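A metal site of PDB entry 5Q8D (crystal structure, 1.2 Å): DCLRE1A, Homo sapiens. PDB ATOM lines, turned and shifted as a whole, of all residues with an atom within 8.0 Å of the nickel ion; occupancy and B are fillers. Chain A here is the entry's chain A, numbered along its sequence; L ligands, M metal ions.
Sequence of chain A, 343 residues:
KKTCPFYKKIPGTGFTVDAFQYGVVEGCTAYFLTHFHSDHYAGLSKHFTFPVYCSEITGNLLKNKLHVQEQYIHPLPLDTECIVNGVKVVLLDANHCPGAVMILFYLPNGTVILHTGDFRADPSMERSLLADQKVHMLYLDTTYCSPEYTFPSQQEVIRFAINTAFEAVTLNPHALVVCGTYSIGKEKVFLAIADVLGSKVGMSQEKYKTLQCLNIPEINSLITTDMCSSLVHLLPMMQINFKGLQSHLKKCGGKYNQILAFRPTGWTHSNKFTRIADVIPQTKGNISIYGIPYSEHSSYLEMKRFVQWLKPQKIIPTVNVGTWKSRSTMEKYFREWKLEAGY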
ATOM      1  N   ASP A  18      28.211 -12.700  -0.616  1.00  0.00           N
ATOM      2  CA  ASP A  18      26.930 -13.026  -1.261  1.00  0.00           C
ATOM      3  C   ASP A  18      25.714 -13.038  -0.233  1.00  0.00           C
ATOM      4  O   ASP A  18      24.833 -13.945  -0.255  1.00  0.00           O
ATOM      5  CB  ASP A  18      27.012 -14.240  -2.107  1.00  0.00           C
ATOM      6  CG  ASP A  18      28.055 -14.139  -3.256  1.00  0.00           C
ATOM      7  OD1 ASP A  18      28.544 -13.047  -3.499  1.00  0.00           O
ATOM      8  OD2 ASP A  18      28.308 -15.240  -3.852  1.00  0.00           O
ATOM      9  N   THR A  34      30.432 -12.050  -5.357  1.00  0.00           N
ATOM     10  CA  THR A  34      31.257 -12.879  -6.265  1.00  0.00           C
ATOM     11  C   THR A  34      30.903 -12.687  -7.750  1.00  0.00           C
ATOM     12  O   THR A  34      31.798 -12.734  -8.623  1.00  0.00           O
ATOM     13  CB  THR A  34      31.279 -14.332  -5.888  1.00  0.00           C
ATOM     14  OG1 THR A  34      29.941 -14.913  -6.055  1.00  0.00           O
ATOM     15  CG2 THR A  34      31.831 -14.629  -4.499  1.00  0.00           C
ATOM     16  N   HIS A  35      29.583 -12.512  -8.047  1.00  0.00           N
ATOM     17  CA  HIS A  35      29.103 -12.431  -9.418  1.00  0.00           C
ATOM     18  C   HIS A  35      27.704 -11.944  -9.489  1.00  0.00           C
ATOM     19  O   HIS A  35      26.941 -12.089  -8.485  1.00  0.00           O
ATOM     20  CB  HIS A  35      29.330 -13.781 -10.190  1.00  0.00           C
ATOM     21  CG  HIS A  35      28.456 -14.923  -9.759  1.00  0.00           C
ATOM     22  ND1 HIS A  35      28.572 -15.585  -8.547  1.00  0.00           N
ATOM     23  CD2 HIS A  35      27.487 -15.603 -10.439  1.00  0.00           C
ATOM     24  CE1 HIS A  35      27.720 -16.603  -8.529  1.00  0.00           C
ATOM     25  NE2 HIS A  35      27.083 -16.633  -9.660  1.00  0.00           N
ATOM     26  N   PHE A  36      27.346 -11.476 -10.690  1.00  0.00           N
ATOM     27  CA  PHE A  36      25.946 -10.921 -10.896  1.00  0.00           C
ATOM     28  C   PHE A  36      24.928 -11.951 -11.316  1.00  0.00           C
ATOM     29  O   PHE A  36      24.447 -11.914 -12.529  1.00  0.00           O
ATOM     30  CB  PHE A  36      26.048  -9.761 -11.900  1.00  0.00           C
ATOM     31  CG  PHE A  36      24.806  -8.858 -11.962  1.00  0.00           C
ATOM     32  CD1 PHE A  36      24.607  -7.910 -10.964  1.00  0.00           C
ATOM     33  CD2 PHE A  36      23.888  -8.941 -12.995  1.00  0.00           C
ATOM     34  CE1 PHE A  36      23.466  -7.043 -11.003  1.00  0.00           C
ATOM     35  CE2 PHE A  36      22.750  -8.098 -13.057  1.00  0.00           C
ATOM     36  CZ  PHE A  36      22.581  -7.158 -12.091  1.00  0.00           C
ATOM     37  N   HIS A  37      24.606 -12.924 -10.443  1.00  0.00           N
ATOM     38  CA  HIS A  37      23.466 -13.838 -10.599  1.00  0.00           C
ATOM     39  C   HIS A  37      22.494 -13.577  -9.421  1.00  0.00           C
ATOM     40  O   HIS A  37      22.907 -13.370  -8.285  1.00  0.00           O
ATOM     41  CB  HIS A  37      23.886 -15.314 -10.660  1.00  0.00           C
ATOM     42  CG  HIS A  37      24.445 -15.786 -11.988  1.00  0.00           C
ATOM     43  ND1 HIS A  37      25.151 -16.977 -12.140  1.00  0.00           N
ATOM     44  CD2 HIS A  37      24.265 -15.292 -13.226  1.00  0.00           C
ATOM     45  CE1 HIS A  37      25.377 -17.192 -13.423  1.00  0.00           C
ATOM     46  NE2 HIS A  37      24.894 -16.149 -14.088  1.00  0.00           N
ATOM     47  N   SER A  38      21.180 -13.655  -9.726  1.00  0.00           N
ATOM     48  CA  SER A  38      20.149 -13.172  -8.779  1.00  0.00           C
ATOM     49  C   SER A  38      20.149 -13.918  -7.475  1.00  0.00           C
ATOM     50  O   SER A  38      19.890 -13.245  -6.442  1.00  0.00           O
ATOM     51  CB  SER A  38      18.769 -13.115  -9.469  1.00  0.00           C
ATOM     52  OG  SER A  38      18.340 -14.392  -9.877  1.00  0.00           O
ATOM     53  N   ASP A  39      20.418 -15.214  -7.420  1.00  0.00           N
ATOM     54  CA  ASP A  39      20.433 -15.948  -6.104  1.00  0.00           C
ATOM     55  C   ASP A  39      21.518 -15.336  -5.207  1.00  0.00           C
ATOM     56  O   ASP A  39      21.404 -15.435  -3.957  1.00  0.00           O
ATOM     57  CB  ASP A  39      20.633 -17.428  -6.188  1.00  0.00           C
ATOM     58  CG  ASP A  39      19.329 -18.245  -6.564  1.00  0.00           C
ATOM     59  OD1 ASP A  39      18.256 -17.633  -6.697  1.00  0.00           O
ATOM     60  OD2 ASP A  39      19.492 -19.474  -6.754  1.00  0.00           O
ATOM     61  N   HIS A  40      22.601 -14.756  -5.794  1.00  0.00           N
ATOM     62  CA  HIS A  40      23.736 -14.206  -5.041  1.00  0.00           C
ATOM     63  C   HIS A  40      23.620 -12.751  -4.730  1.00  0.00           C
ATOM     64  O   HIS A  40      24.014 -12.325  -3.596  1.00  0.00           O
ATOM     65  CB  HIS A  40      25.057 -14.514  -5.828  1.00  0.00           C
ATOM     66  CG  HIS A  40      25.303 -15.952  -5.972  1.00  0.00           C
ATOM     67  ND1 HIS A  40      26.218 -16.654  -5.215  1.00  0.00           N
ATOM     68  CD2 HIS A  40      24.718 -16.879  -6.775  1.00  0.00           C
ATOM     69  CE1 HIS A  40      26.168 -17.933  -5.517  1.00  0.00           C
ATOM     70  NE2 HIS A  40      25.252 -18.101  -6.467  1.00  0.00           N
ATOM     71  N   HIS A  96      33.328 -18.788 -14.573  1.00  0.00           N
ATOM     72  CA  HIS A  96      31.860 -18.910 -14.454  1.00  0.00           C
ATOM     73  C   HIS A  96      31.288 -17.980 -15.503  1.00  0.00           C
ATOM     74  O   HIS A  96      31.485 -18.275 -16.720  1.00  0.00           O
ATOM     75  CB  HIS A  96      31.420 -18.704 -12.990  1.00  0.00           C
ATOM     76  CG  HIS A  96      29.950 -18.909 -12.673  1.00  0.00           C
ATOM     77  ND1 HIS A  96      29.285 -20.062 -12.994  1.00  0.00           N
ATOM     78  CD2 HIS A  96      29.037 -18.092 -12.079  1.00  0.00           C
ATOM     79  CE1 HIS A  96      28.009 -19.919 -12.598  1.00  0.00           C
ATOM     80  NE2 HIS A  96      27.830 -18.755 -11.998  1.00  0.00           N
ATOM     81  N   CYS A  97      30.496 -17.003 -15.169  1.00  0.00           N
ATOM     82  CA  CYS A  97      29.972 -15.951 -16.092  1.00  0.00           C
ATOM     83  C   CYS A  97      30.889 -14.740 -16.102  1.00  0.00           C
ATOM     84  O   CYS A  97      31.780 -14.618 -15.263  1.00  0.00           O
ATOM     85  CB  CYS A  97      28.546 -15.604 -15.623  1.00  0.00           C
ATOM     86  SG  CYS A  97      28.443 -14.792 -13.982  1.00  0.00           S
ATOM     87  N   ALA A 100      32.705 -12.923 -12.825  1.00  0.00           N
ATOM     88  CA  ALA A 100      32.665 -13.831 -11.662  1.00  0.00           C
ATOM     89  C   ALA A 100      34.056 -14.064 -11.124  1.00  0.00           C
ATOM     90  O   ALA A 100      35.017 -14.331 -11.897  1.00  0.00           O
ATOM     91  CB  ALA A 100      32.033 -15.159 -12.017  1.00  0.00           C
ATOM     92  N   GLY A 117      33.145 -18.756  -4.818  1.00  0.00           N
ATOM     93  CA  GLY A 117      31.909 -18.312  -5.435  1.00  0.00           C
ATOM     94  C   GLY A 117      31.316 -19.461  -6.223  1.00  0.00           C
ATOM     95  O   GLY A 117      31.405 -20.610  -5.813  1.00  0.00           O
ATOM     96  N   ASP A 118      30.678 -19.152  -7.343  1.00  0.00           N
ATOM     97  CA  ASP A 118      30.366 -20.167  -8.386  1.00  0.00           C
ATOM     98  C   ASP A 118      31.582 -20.281  -9.341  1.00  0.00           C
ATOM     99  O   ASP A 118      32.125 -19.249  -9.768  1.00  0.00           O
ATOM    100  CB  ASP A 118      29.115 -19.849  -9.179  1.00  0.00           C
ATOM    101  CG  ASP A 118      27.780 -20.091  -8.430  1.00  0.00           C
ATOM    102  OD1 ASP A 118      27.767 -20.712  -7.347  1.00  0.00           O
ATOM    103  OD2 ASP A 118      26.738 -19.707  -8.994  1.00  0.00           O
ATOM    104  N   PHE A 119      31.980 -21.519  -9.670  1.00  0.00           N
ATOM    105  CA  PHE A 119      33.156 -21.693 -10.556  1.00  0.00           C
ATOM    106  C   PHE A 119      33.042 -22.938 -11.403  1.00  0.00           C
ATOM    107  O   PHE A 119      32.335 -23.891 -11.055  1.00  0.00           O
ATOM    108  CB  PHE A 119      34.545 -21.625  -9.775  1.00  0.00           C
ATOM    109  CG  PHE A 119      35.064 -22.911  -9.099  1.00  0.00           C
ATOM    110  CD1 PHE A 119      36.419 -23.196  -9.110  1.00  0.00           C
ATOM    111  CD2 PHE A 119      34.214 -23.802  -8.378  1.00  0.00           C
ATOM    112  CE1 PHE A 119      36.921 -24.313  -8.441  1.00  0.00           C
ATOM    113  CE2 PHE A 119      34.722 -24.925  -7.745  1.00  0.00           C
ATOM    114  CZ  PHE A 119      36.072 -25.152  -7.756  1.00  0.00           C
ATOM    115  N   ASP A 141      31.942 -24.336  -4.259  1.00  0.00           N
ATOM    116  CA  ASP A 141      30.727 -24.521  -5.142  1.00  0.00           C
ATOM    117  C   ASP A 141      30.628 -26.009  -5.447  1.00  0.00           C
ATOM    118  O   ASP A 141      31.308 -26.564  -6.307  1.00  0.00           O
ATOM    119  CB  ASP A 141      30.867 -23.698  -6.415  1.00  0.00           C
ATOM    120  CG  ASP A 141      29.857 -24.033  -7.481  1.00  0.00           C
ATOM    121  OD1 ASP A 141      28.827 -24.719  -7.162  1.00  0.00           O
ATOM    122  OD2 ASP A 141      30.075 -23.597  -8.659  1.00  0.00           O
ATOM    123  N   THR A 143      27.785 -27.537  -6.598  1.00  0.00           N
ATOM    124  CA  THR A 143      26.599 -27.751  -7.422  1.00  0.00           C
ATOM    125  C   THR A 143      26.499 -29.152  -7.978  1.00  0.00           C
ATOM    126  O   THR A 143      25.415 -29.826  -7.798  1.00  0.00           O
ATOM    127  CB  THR A 143      26.548 -26.695  -8.587  1.00  0.00           C
ATOM    128  OG1 THR A 143      26.417 -25.370  -8.091  1.00  0.00           O
ATOM    129  CG2 THR A 143      25.340 -26.950  -9.514  1.00  0.00           C
ATOM    130  N   SER A 183      19.855 -14.889 -17.774  1.00  0.00           N
ATOM    131  CA  SER A 183      20.867 -14.325 -16.879  1.00  0.00           C
ATOM    132  C   SER A 183      22.100 -14.053 -17.748  1.00  0.00           C
ATOM    133  O   SER A 183      22.188 -14.530 -18.924  1.00  0.00           O
ATOM    134  CB  SER A 183      21.275 -15.325 -15.767  1.00  0.00           C
ATOM    135  OG  SER A 183      21.779 -16.529 -16.315  1.00  0.00           O
ATOM    136  N   ILE A 184      23.108 -13.414 -17.209  1.00  0.00           N
ATOM    137  CA  ILE A 184      24.408 -13.405 -17.861  1.00  0.00           C
ATOM    138  C   ILE A 184      25.090 -14.777 -17.765  1.00  0.00           C
ATOM    139  O   ILE A 184      24.695 -15.658 -16.938  1.00  0.00           O
ATOM    140  CB  ILE A 184      25.380 -12.295 -17.312  1.00  0.00           C
ATOM    141  CG1 ILE A 184      25.788 -12.497 -15.855  1.00  0.00           C
ATOM    142  CG2 ILE A 184      24.738 -10.908 -17.512  1.00  0.00           C
ATOM    143  CD1 ILE A 184      26.963 -11.640 -15.392  1.00  0.00           C
ATOM    144  N   GLU A 296      28.558 -23.826 -16.862  1.00  0.00           N
ATOM    145  CA  GLU A 296      29.499 -22.916 -16.201  1.00  0.00           C
ATOM    146  C   GLU A 296      29.825 -23.282 -14.713  1.00  0.00           C
ATOM    147  O   GLU A 296      30.288 -22.455 -13.908  1.00  0.00           O
ATOM    148  CB  GLU A 296      29.094 -21.458 -16.377  1.00  0.00           C
ATOM    149  CG  GLU A 296      29.237 -20.975 -17.877  1.00  0.00           C
ATOM    150  CD  GLU A 296      28.992 -19.483 -18.154  1.00  0.00           C
ATOM    151  OE1 GLU A 296      28.315 -18.797 -17.359  1.00  0.00           O
ATOM    152  OE2 GLU A 296      29.451 -19.033 -19.284  1.00  0.00           O
ATOM    153  N   HIS A 297      29.495 -24.539 -14.370  1.00  0.00           N
ATOM    154  CA  HIS A 297      29.914 -25.129 -13.084  1.00  0.00           C
ATOM    155  C   HIS A 297      30.800 -26.372 -13.311  1.00  0.00           C
ATOM    156  O   HIS A 297      30.654 -27.072 -14.317  1.00  0.00           O
ATOM    157  CB  HIS A 297      28.687 -25.550 -12.230  1.00  0.00           C
ATOM    158  CG  HIS A 297      27.816 -24.452 -11.756  1.00  0.00           C
ATOM    159  ND1 HIS A 297      28.029 -23.716 -10.597  1.00  0.00           N
ATOM    160  CD2 HIS A 297      26.631 -24.014 -12.262  1.00  0.00           C
ATOM    161  CE1 HIS A 297      27.045 -22.843 -10.461  1.00  0.00           C
ATOM    162  NE2 HIS A 297      26.198 -23.010 -11.452  1.00  0.00           N
HETATM  163  C1  LIG L   1      22.942 -19.592 -11.073  1.00  0.00           C
HETATM  164  C2  LIG L   1      24.002 -20.579 -11.571  1.00  0.00           C
HETATM  165  C3  LIG L   1      23.259 -18.943  -9.704  1.00  0.00           C
HETATM  166  O1  LIG L   1      23.769 -21.708 -12.005  1.00  0.00           O
HETATM  167  O2  LIG L   1      25.139 -20.140 -11.559  1.00  0.00           O
HETATM  168  O3  LIG L   1      24.353 -18.360  -9.493  1.00  0.00           O
HETATM  169  O4  LIG L   1      22.305 -18.935  -8.845  1.00  0.00           O
HETATM  170 NI    NI M   1      26.060 -18.390 -10.638  1.00  0.00          NI
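O3 of the ligand is bound to the nickel ion (2.1 Å). O2 of the ligand binds the nickel ion, 2.2 Å away. The nickel ion is bound by OD2 of Asp 118, 2.2 Å away. A ring nitrogen (ND1) of His 37 is bound to the nickel ion, at 2.3 Å. A ring nitrogen (NE2) of His 35 binds the nickel ion, at 2.3 Å. A ring nitrogen (NE2) of His 96 binds the nickel ion (2.3 Å).
A ring nitrogen (NE2) of His 40 sits close to the side-chain carboxylate (OD2) of Asp 118, 3.3 Å away. The side-chain hydroxyl (OG1) of Thr 34 sits at hydrogen-bond distance from a ring nitrogen (ND1) of His 35 (2.9 Å). A ring nitrogen (ND1) of His 96 is in hydrogen-bond range of the backbone carbonyl oxygen (O) of Glu 296 (2.8 Å). O of Ile 184 is in hydrogen-bond range of NE2 of His 37, 2.9 Å away.
Within 4 Å of the nickel ion: His 35, His 37, His 96 and Asp 118. The nearest printed residue that does not touch the nickel ion is His 40 (4.3 Å).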
